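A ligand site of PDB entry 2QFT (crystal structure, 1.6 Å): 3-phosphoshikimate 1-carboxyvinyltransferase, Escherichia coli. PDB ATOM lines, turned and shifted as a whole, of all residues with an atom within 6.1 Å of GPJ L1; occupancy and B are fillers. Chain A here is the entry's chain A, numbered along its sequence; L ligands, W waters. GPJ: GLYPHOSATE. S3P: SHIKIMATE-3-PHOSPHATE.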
ATOM      1  N   LYS A  22     -15.788 -20.826  -9.621  1.00  0.00           N
ATOM      2  CA  LYS A  22     -16.706 -21.418  -8.649  1.00  0.00           C
ATOM      3  C   LYS A  22     -16.717 -20.566  -7.359  1.00  0.00           C
ATOM      4  O   LYS A  22     -17.781 -20.285  -6.811  1.00  0.00           O
ATOM      5  CB  LYS A  22     -16.265 -22.864  -8.340  1.00  0.00           C
ATOM      6  CG  LYS A  22     -17.059 -23.548  -7.206  1.00  0.00           C
ATOM      7  CD  LYS A  22     -16.211 -23.845  -5.954  1.00  0.00           C
ATOM      8  CE  LYS A  22     -15.277 -25.033  -6.205  1.00  0.00           C
ATOM      9  NZ  LYS A  22     -14.260 -25.182  -5.128  1.00  0.00           N
ATOM     10  N   ASP A  49     -21.478 -27.448  -8.066  1.00  0.00           N
ATOM     11  CA  ASP A  49     -21.384 -26.615  -6.866  1.00  0.00           C
ATOM     12  C   ASP A  49     -22.232 -25.351  -6.946  1.00  0.00           C
ATOM     13  O   ASP A  49     -22.795 -24.917  -5.929  1.00  0.00           O
ATOM     14  CB  ASP A  49     -19.929 -26.239  -6.560  1.00  0.00           C
ATOM     15  CG  ASP A  49     -19.148 -27.388  -5.919  1.00  0.00           C
ATOM     16  OD1 ASP A  49     -19.717 -28.470  -5.692  1.00  0.00           O
ATOM     17  OD2 ASP A  49     -17.957 -27.167  -5.625  1.00  0.00           O
ATOM     18  N   ASN A  94     -21.537 -31.785  -2.618  1.00  0.00           N
ATOM     19  CA  ASN A  94     -20.293 -31.807  -1.844  1.00  0.00           C
ATOM     20  C   ASN A  94     -19.656 -30.432  -2.021  1.00  0.00           C
ATOM     21  O   ASN A  94     -18.434 -30.296  -2.074  1.00  0.00           O
ATOM     22  CB  ASN A  94     -19.345 -32.910  -2.327  1.00  0.00           C
ATOM     23  CG  ASN A  94     -18.215 -33.176  -1.327  1.00  0.00           C
ATOM     24  OD1 ASN A  94     -18.301 -32.777  -0.169  1.00  0.00           O
ATOM     25  ND2 ASN A  94     -17.185 -33.908  -1.760  1.00  0.00           N
ATOM     26  N   ALA A  95     -20.516 -29.414  -2.081  1.00  0.00           N
ATOM     27  CA  ALA A  95     -20.059 -28.031  -2.267  1.00  0.00           C
ATOM     28  C   ALA A  95     -19.743 -27.323  -0.956  1.00  0.00           C
ATOM     29  O   ALA A  95     -20.634 -26.770  -0.311  1.00  0.00           O
ATOM     30  CB  ALA A  95     -21.137 -27.239  -3.040  1.00  0.00           C
ATOM     31  N   GLY A  96     -18.470 -27.333  -0.566  1.00  0.00           N
ATOM     32  CA  GLY A  96     -18.095 -26.663   0.667  1.00  0.00           C
ATOM     33  C   GLY A  96     -18.416 -25.178   0.625  1.00  0.00           C
ATOM     34  O   GLY A  96     -18.837 -24.602   1.638  1.00  0.00           O
ATOM     35  N   THR A  97     -18.226 -24.531  -0.519  1.00  0.00           N
ATOM     36  CA  THR A  97     -18.475 -23.096  -0.606  1.00  0.00           C
ATOM     37  C   THR A  97     -19.924 -22.780  -0.293  1.00  0.00           C
ATOM     38  O   THR A  97     -20.209 -21.691   0.203  1.00  0.00           O
ATOM     39  CB  THR A  97     -18.088 -22.502  -1.990  1.00  0.00           C
ATOM     40  OG1 THR A  97     -18.795 -23.193  -3.031  1.00  0.00           O
ATOM     41  CG2 THR A  97     -16.594 -22.608  -2.218  1.00  0.00           C
ATOM     42  N   ARG A 100     -20.540 -24.259   3.885  1.00  0.00           N
ATOM     43  CA  ARG A 100     -19.993 -23.405   4.924  1.00  0.00           C
ATOM     44  C   ARG A 100     -20.642 -22.027   4.926  1.00  0.00           C
ATOM     45  O   ARG A 100     -21.102 -21.561   5.979  1.00  0.00           O
ATOM     46  CB  ARG A 100     -18.467 -23.286   4.794  1.00  0.00           C
ATOM     47  CG  ARG A 100     -17.658 -24.487   5.371  1.00  0.00           C
ATOM     48  CD  ARG A 100     -17.890 -25.798   4.587  1.00  0.00           C
ATOM     49  NE  ARG A 100     -17.091 -26.928   5.107  1.00  0.00           N
ATOM     50  CZ  ARG A 100     -15.885 -27.265   4.671  1.00  0.00           C
ATOM     51  NH1 ARG A 100     -15.245 -28.307   5.205  1.00  0.00           N
ATOM     52  NH2 ARG A 100     -15.304 -26.562   3.689  1.00  0.00           N
ATOM     53  N   MET A 121     -19.712 -35.342   2.038  1.00  0.00           N
ATOM     54  CA  MET A 121     -19.855 -34.076   2.754  1.00  0.00           C
ATOM     55  C   MET A 121     -20.132 -34.288   4.232  1.00  0.00           C
ATOM     56  O   MET A 121     -19.755 -33.445   5.063  1.00  0.00           O
ATOM     57  CB  MET A 121     -20.975 -33.225   2.106  1.00  0.00           C
ATOM     58  CG  MET A 121     -21.292 -31.919   2.844  1.00  0.00           C
ATOM     59  SD  MET A 121     -19.882 -30.778   3.081  1.00  0.00           S
ATOM     60  CE  MET A 121     -19.718 -30.053   1.429  1.00  0.00           C
ATOM     61  N   ARG A 124     -16.807 -34.259   5.945  1.00  0.00           N
ATOM     62  CA  ARG A 124     -15.944 -33.079   5.821  1.00  0.00           C
ATOM     63  C   ARG A 124     -16.247 -32.203   7.031  1.00  0.00           C
ATOM     64  O   ARG A 124     -17.398 -31.835   7.262  1.00  0.00           O
ATOM     65  CB  ARG A 124     -16.195 -32.373   4.495  1.00  0.00           C
ATOM     66  CG  ARG A 124     -15.714 -33.226   3.285  1.00  0.00           C
ATOM     67  CD  ARG A 124     -15.878 -32.485   1.991  1.00  0.00           C
ATOM     68  NE  ARG A 124     -15.055 -31.281   1.970  1.00  0.00           N
ATOM     69  CZ  ARG A 124     -15.227 -30.269   1.119  1.00  0.00           C
ATOM     70  NH1 ARG A 124     -14.435 -29.217   1.186  1.00  0.00           N
ATOM     71  NH2 ARG A 124     -16.185 -30.312   0.194  1.00  0.00           N
ATOM     72  N   GLN A 171     -12.675 -21.395   4.722  1.00  0.00           N
ATOM     73  CA  GLN A 171     -14.111 -21.212   4.493  1.00  0.00           C
ATOM     74  C   GLN A 171     -14.918 -20.866   5.724  1.00  0.00           C
ATOM     75  O   GLN A 171     -15.979 -20.242   5.622  1.00  0.00           O
ATOM     76  CB  GLN A 171     -14.715 -22.450   3.820  1.00  0.00           C
ATOM     77  CG  GLN A 171     -14.191 -22.650   2.402  1.00  0.00           C
ATOM     78  CD  GLN A 171     -14.924 -23.737   1.688  1.00  0.00           C
ATOM     79  OE1 GLN A 171     -15.916 -24.287   2.198  1.00  0.00           O
ATOM     80  NE2 GLN A 171     -14.462 -24.068   0.473  1.00  0.00           N
ATOM     81  N   ASP A 313      -5.580 -25.982  -4.374  1.00  0.00           N
ATOM     82  CA  ASP A 313      -6.328 -26.663  -5.434  1.00  0.00           C
ATOM     83  C   ASP A 313      -5.496 -26.808  -6.708  1.00  0.00           C
ATOM     84  O   ASP A 313      -5.324 -27.920  -7.237  1.00  0.00           O
ATOM     85  CB  ASP A 313      -7.632 -25.908  -5.751  1.00  0.00           C
ATOM     86  CG  ASP A 313      -8.617 -25.908  -4.577  1.00  0.00           C
ATOM     87  OD1 ASP A 313      -9.657 -25.236  -4.711  1.00  0.00           O
ATOM     88  OD2 ASP A 313      -8.356 -26.546  -3.531  1.00  0.00           O
ATOM     89  N   MET A 316      -2.552 -29.426  -7.001  1.00  0.00           N
ATOM     90  CA  MET A 316      -2.720 -30.820  -7.448  1.00  0.00           C
ATOM     91  C   MET A 316      -2.232 -30.975  -8.870  1.00  0.00           C
ATOM     92  O   MET A 316      -1.708 -32.028  -9.236  1.00  0.00           O
ATOM     93  CB  MET A 316      -4.182 -31.251  -7.351  1.00  0.00           C
ATOM     94  CG  MET A 316      -4.794 -31.202  -5.957  1.00  0.00           C
ATOM     95  SD  MET A 316      -6.548 -31.692  -6.000  1.00  0.00           S
ATOM     96  CE  MET A 316      -6.445 -33.479  -6.531  1.00  0.00           C
ATOM     97  N   LYS A 340     -10.956 -32.616   1.807  1.00  0.00           N
ATOM     98  CA  LYS A 340     -11.728 -32.035   0.708  1.00  0.00           C
ATOM     99  C   LYS A 340     -12.568 -33.071  -0.063  1.00  0.00           C
ATOM    100  O   LYS A 340     -13.116 -33.962   0.580  1.00  0.00           O
ATOM    101  CB  LYS A 340     -10.808 -31.194  -0.190  1.00  0.00           C
ATOM    102  CG  LYS A 340     -10.463 -29.870   0.552  1.00  0.00           C
ATOM    103  CD  LYS A 340      -9.373 -29.063  -0.112  1.00  0.00           C
ATOM    104  CE  LYS A 340      -9.312 -27.691   0.586  1.00  0.00           C
ATOM    105  NZ  LYS A 340      -8.111 -26.914   0.179  1.00  0.00           N
ATOM    106  N   GLU A 341     -12.676 -32.982  -1.390  1.00  0.00           N
ATOM    107  CA  GLU A 341     -13.541 -33.927  -2.116  1.00  0.00           C
ATOM    108  C   GLU A 341     -13.302 -35.390  -1.804  1.00  0.00           C
ATOM    109  O   GLU A 341     -14.230 -36.209  -1.828  1.00  0.00           O
ATOM    110  CB  GLU A 341     -13.490 -33.660  -3.619  1.00  0.00           C
ATOM    111  CG  GLU A 341     -14.307 -32.403  -4.016  1.00  0.00           C
ATOM    112  CD  GLU A 341     -13.570 -31.075  -3.839  1.00  0.00           C
ATOM    113  OE1 GLU A 341     -12.602 -30.991  -3.034  1.00  0.00           O
ATOM    114  OE2 GLU A 341     -13.981 -30.101  -4.495  1.00  0.00           O
ATOM    115  N   ARG A 344      -7.131 -36.246  -0.665  1.00  0.00           N
ATOM    116  CA  ARG A 344      -6.305 -36.068  -1.858  1.00  0.00           C
ATOM    117  C   ARG A 344      -4.846 -36.489  -1.739  1.00  0.00           C
ATOM    118  O   ARG A 344      -4.214 -36.810  -2.746  1.00  0.00           O
ATOM    119  CB  ARG A 344      -6.434 -34.605  -2.335  1.00  0.00           C
ATOM    120  CG  ARG A 344      -7.838 -34.335  -2.884  1.00  0.00           C
ATOM    121  CD  ARG A 344      -8.107 -32.842  -3.006  1.00  0.00           C
ATOM    122  NE  ARG A 344      -9.111 -32.603  -4.041  1.00  0.00           N
ATOM    123  CZ  ARG A 344      -9.506 -31.396  -4.434  1.00  0.00           C
ATOM    124  NH1 ARG A 344     -10.406 -31.274  -5.418  1.00  0.00           N
ATOM    125  NH2 ARG A 344      -9.016 -30.308  -3.847  1.00  0.00           N
ATOM    126  N   ASP A 384     -13.940 -36.966  -7.323  1.00  0.00           N
ATOM    127  CA  ASP A 384     -13.186 -35.731  -7.231  1.00  0.00           C
ATOM    128  C   ASP A 384     -12.811 -35.171  -8.605  1.00  0.00           C
ATOM    129  O   ASP A 384     -11.880 -35.661  -9.249  1.00  0.00           O
ATOM    130  CB  ASP A 384     -11.924 -35.974  -6.390  1.00  0.00           C
ATOM    131  CG  ASP A 384     -11.098 -34.708  -6.144  1.00  0.00           C
ATOM    132  OD1 ASP A 384     -11.431 -33.635  -6.716  1.00  0.00           O
ATOM    133  OD2 ASP A 384     -10.100 -34.802  -5.391  1.00  0.00           O
ATOM    134  N   HIS A 385     -13.552 -34.142  -9.022  1.00  0.00           N
ATOM    135  CA  HIS A 385     -13.290 -33.460 -10.290  1.00  0.00           C
ATOM    136  C   HIS A 385     -11.798 -33.256 -10.584  1.00  0.00           C
ATOM    137  O   HIS A 385     -11.339 -33.490 -11.715  1.00  0.00           O
ATOM    138  CB  HIS A 385     -14.012 -32.091 -10.324  1.00  0.00           C
ATOM    139  CG  HIS A 385     -13.670 -31.182  -9.177  1.00  0.00           C
ATOM    140  ND1 HIS A 385     -13.462 -29.827  -9.353  1.00  0.00           N
ATOM    141  CD2 HIS A 385     -13.556 -31.411  -7.846  1.00  0.00           C
ATOM    142  CE1 HIS A 385     -13.227 -29.266  -8.182  1.00  0.00           C
ATOM    143  NE2 HIS A 385     -13.275 -30.194  -7.248  1.00  0.00           N
ATOM    144  N   ARG A 386     -11.019 -32.855  -9.585  1.00  0.00           N
ATOM    145  CA  ARG A 386      -9.613 -32.609  -9.863  1.00  0.00           C
ATOM    146  C   ARG A 386      -8.758 -33.847 -10.072  1.00  0.00           C
ATOM    147  O   ARG A 386      -7.722 -33.758 -10.713  1.00  0.00           O
ATOM    148  CB  ARG A 386      -8.992 -31.680  -8.799  1.00  0.00           C
ATOM    149  CG  ARG A 386      -9.685 -30.301  -8.770  1.00  0.00           C
ATOM    150  CD  ARG A 386      -8.789 -29.163  -8.187  1.00  0.00           C
ATOM    151  NE  ARG A 386      -9.682 -28.054  -7.887  1.00  0.00           N
ATOM    152  CZ  ARG A 386     -10.240 -27.267  -8.798  1.00  0.00           C
ATOM    153  NH1 ARG A 386     -11.099 -26.326  -8.394  1.00  0.00           N
ATOM    154  NH2 ARG A 386      -9.903 -27.345 -10.086  1.00  0.00           N
ATOM    155  N   LYS A 411     -18.330 -31.134 -11.089  1.00  0.00           N
ATOM    156  CA  LYS A 411     -18.395 -30.376  -9.826  1.00  0.00           C
ATOM    157  C   LYS A 411     -18.042 -28.905 -10.090  1.00  0.00           C
ATOM    158  O   LYS A 411     -18.667 -28.001  -9.532  1.00  0.00           O
ATOM    159  CB  LYS A 411     -17.465 -30.971  -8.758  1.00  0.00           C
ATOM    160  CG  LYS A 411     -17.697 -30.348  -7.383  1.00  0.00           C
ATOM    161  CD  LYS A 411     -17.044 -31.166  -6.250  1.00  0.00           C
ATOM    162  CE  LYS A 411     -17.446 -30.664  -4.861  1.00  0.00           C
ATOM    163  NZ  LYS A 411     -16.776 -29.373  -4.462  1.00  0.00           N
ATOM    164  N   THR A 412     -17.056 -28.663 -10.958  1.00  0.00           N
ATOM    165  CA  THR A 412     -16.619 -27.315 -11.314  1.00  0.00           C
ATOM    166  C   THR A 412     -16.379 -27.079 -12.794  1.00  0.00           C
ATOM    167  O   THR A 412     -16.222 -25.937 -13.199  1.00  0.00           O
ATOM    168  CB  THR A 412     -15.270 -26.946 -10.652  1.00  0.00           C
ATOM    169  OG1 THR A 412     -14.246 -27.856 -11.119  1.00  0.00           O
ATOM    170  CG2 THR A 412     -15.362 -26.979  -9.137  1.00  0.00           C
HETATM  171  P1  GPJ L   1     -15.037 -27.205  -1.579  1.00  0.00           P
HETATM  172  O1  GPJ L   1     -15.190 -26.082  -2.538  1.00  0.00           O
HETATM  173  O2  GPJ L   1     -15.024 -26.769  -0.146  1.00  0.00           O
HETATM  174  O3  GPJ L   1     -16.050 -28.266  -1.821  1.00  0.00           O
HETATM  175  O4  GPJ L   1     -12.215 -27.248  -5.675  1.00  0.00           O
HETATM  176  O5  GPJ L   1     -10.298 -28.326  -5.434  1.00  0.00           O
HETATM  177  C1  GPJ L   1     -13.469 -27.891  -1.788  1.00  0.00           C
HETATM  178  C2  GPJ L   1     -11.668 -28.234  -3.537  1.00  0.00           C
HETATM  179  C3  GPJ L   1     -11.364 -27.914  -4.991  1.00  0.00           C
HETATM  180  N1  GPJ L   1     -12.995 -27.727  -3.153  1.00  0.00           N
HETATM  181  C1  S3P L   2     -12.538 -21.997  -1.428  1.00  0.00           C
HETATM  182  C2  S3P L   2     -11.541 -22.143  -0.436  1.00  0.00           C
HETATM  183  C3  S3P L   2     -10.622 -23.361  -0.421  1.00  0.00           C
HETATM  184  C4  S3P L   2     -10.629 -24.140  -1.762  1.00  0.00           C
HETATM  185  C5  S3P L   2     -12.070 -24.351  -2.269  1.00  0.00           C
HETATM  186  C6  S3P L   2     -12.707 -22.976  -2.483  1.00  0.00           C
HETATM  187  C7  S3P L   2     -13.424 -20.783  -1.387  1.00  0.00           C
HETATM  188  O1  S3P L   2     -10.916 -24.229   0.711  1.00  0.00           O
HETATM  189  O2  S3P L   2      -9.899 -25.367  -1.595  1.00  0.00           O
HETATM  190  O3  S3P L   2     -12.072 -25.080  -3.508  1.00  0.00           O
HETATM  191  O4  S3P L   2     -13.606 -20.221  -0.266  1.00  0.00           O
HETATM  192  O5  S3P L   2     -13.907 -20.390  -2.455  1.00  0.00           O
HETATM  193  P1  S3P L   2     -10.023 -24.289   2.073  1.00  0.00           P
HETATM  194  O6  S3P L   2     -10.060 -22.925   2.690  1.00  0.00           O
HETATM  195  O7  S3P L   2      -8.604 -24.687   1.679  1.00  0.00           O
HETATM  196  O8  S3P L   2     -10.676 -25.310   2.945  1.00  0.00           O
HETATM  197  O   HOH W   1     -12.931 -26.715   1.960  1.00  0.00           O
HETATM  198  O   HOH W   2     -17.689 -25.640  -3.366  1.00  0.00           O
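N of Gly 96 lies within hydrogen-bond range of O3 of GPJ L1 (2.9 Å).
The guanidinium group of Arg 100 lies within salt-bridge range of an oxygen (O2) of GPJ L1, at 3.9 Å.
O5 of GPJ L1 is in salt-bridge range of NH2 of Arg 344 (2.8 Å).
An oxygen (O3) of S3P L2 is in hydrogen-bond range of the side-chain amino group (NZ) of Lys 22, at 2.7 Å.
NE2 of Gln 171 is in hydrogen-bond range of O2 of GPJ L1, 2.8 Å away.
NE of Arg 386 lies within salt-bridge range of O5 of GPJ L1, 2.5 Å away.
O2 of GPJ L1 lies within salt-bridge range of NH1 of Arg 124 (2.8 Å).
An oxygen (O1) of GPJ L1 lies within salt-bridge range of the side-chain amino group (NZ) of Lys 22 (2.9 Å).
NZ of Lys 411 lies within salt-bridge range of O3 of GPJ L1, 3.0 Å away.
An oxygen (O3) of S3P L2 is in hydrogen-bond range of the side-chain carboxylate (OD1) of Asp 313, at 2.7 Å.
OE2 of Glu 341 lies within salt-bridge range of N1 of GPJ L1, at 2.9 Å.
O7 of S3P L2 is in salt-bridge range of NZ of Lys 340 (2.7 Å).
The backbone NH of Arg 386 is in hydrogen-bond range of the side-chain carboxylate of Asp 384 (3.0 Å).
The side-chain amide oxygen of Gln 171 is in hydrogen-bond range of the guanidinium group of Arg 100 (2.8 Å).
The side-chain carboxylate (OE2) of Glu 341 sits at hydrogen-bond distance from a ring nitrogen (NE2) of His 385 (2.8 Å).
NZ of Lys 411 lies within salt-bridge range of OE2 of Glu 341.
The side-chain carboxylate of Asp 384 lies within salt-bridge range of the guanidinium group of Arg 344 (2.8 Å).
OD2 of Asp 49 is in salt-bridge range of NZ of Lys 411, 2.8 Å away.
The guanidinium group (NE) of Arg 344 lies within hydrogen-bond range of the side-chain sulfur (SD) of Met 316 (3.4 Å).
The side-chain carboxylate (OD2) of Asp 313 is in salt-bridge range of the side-chain amino group (NZ) of Lys 340 (3.7 Å).
O3 of S3P L2 lies within hydrogen-bond range of N1 of GPJ L1 (2.8 Å).
The backbone carbonyl oxygen (O) of Asn 94 sits close to an oxygen (O3) of GPJ L1 (3.1 Å).
The side-chain carboxylate of Asp 313 sits close to an oxygen (O5) of GPJ L1.
C of Ala 95 touches O3 of GPJ L1 (3.9 Å).
CG2 of Thr 97 touches O1 of GPJ L1, at 3.8 Å.
His 385 touches GPJ L1 (CE1 to O4, 3.4 Å).
Hydrophobic or aromatic side chains within 4 Å of GPJ L1: His 385.
Water W2 lies within hydrogen-bond range of O1 of GPJ L1 (2.7 Å), OG1 of Thr 97 (2.7 Å), OD2 of Asp 49 (2.7 Å) and N of Gly 96 (3.4 Å).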
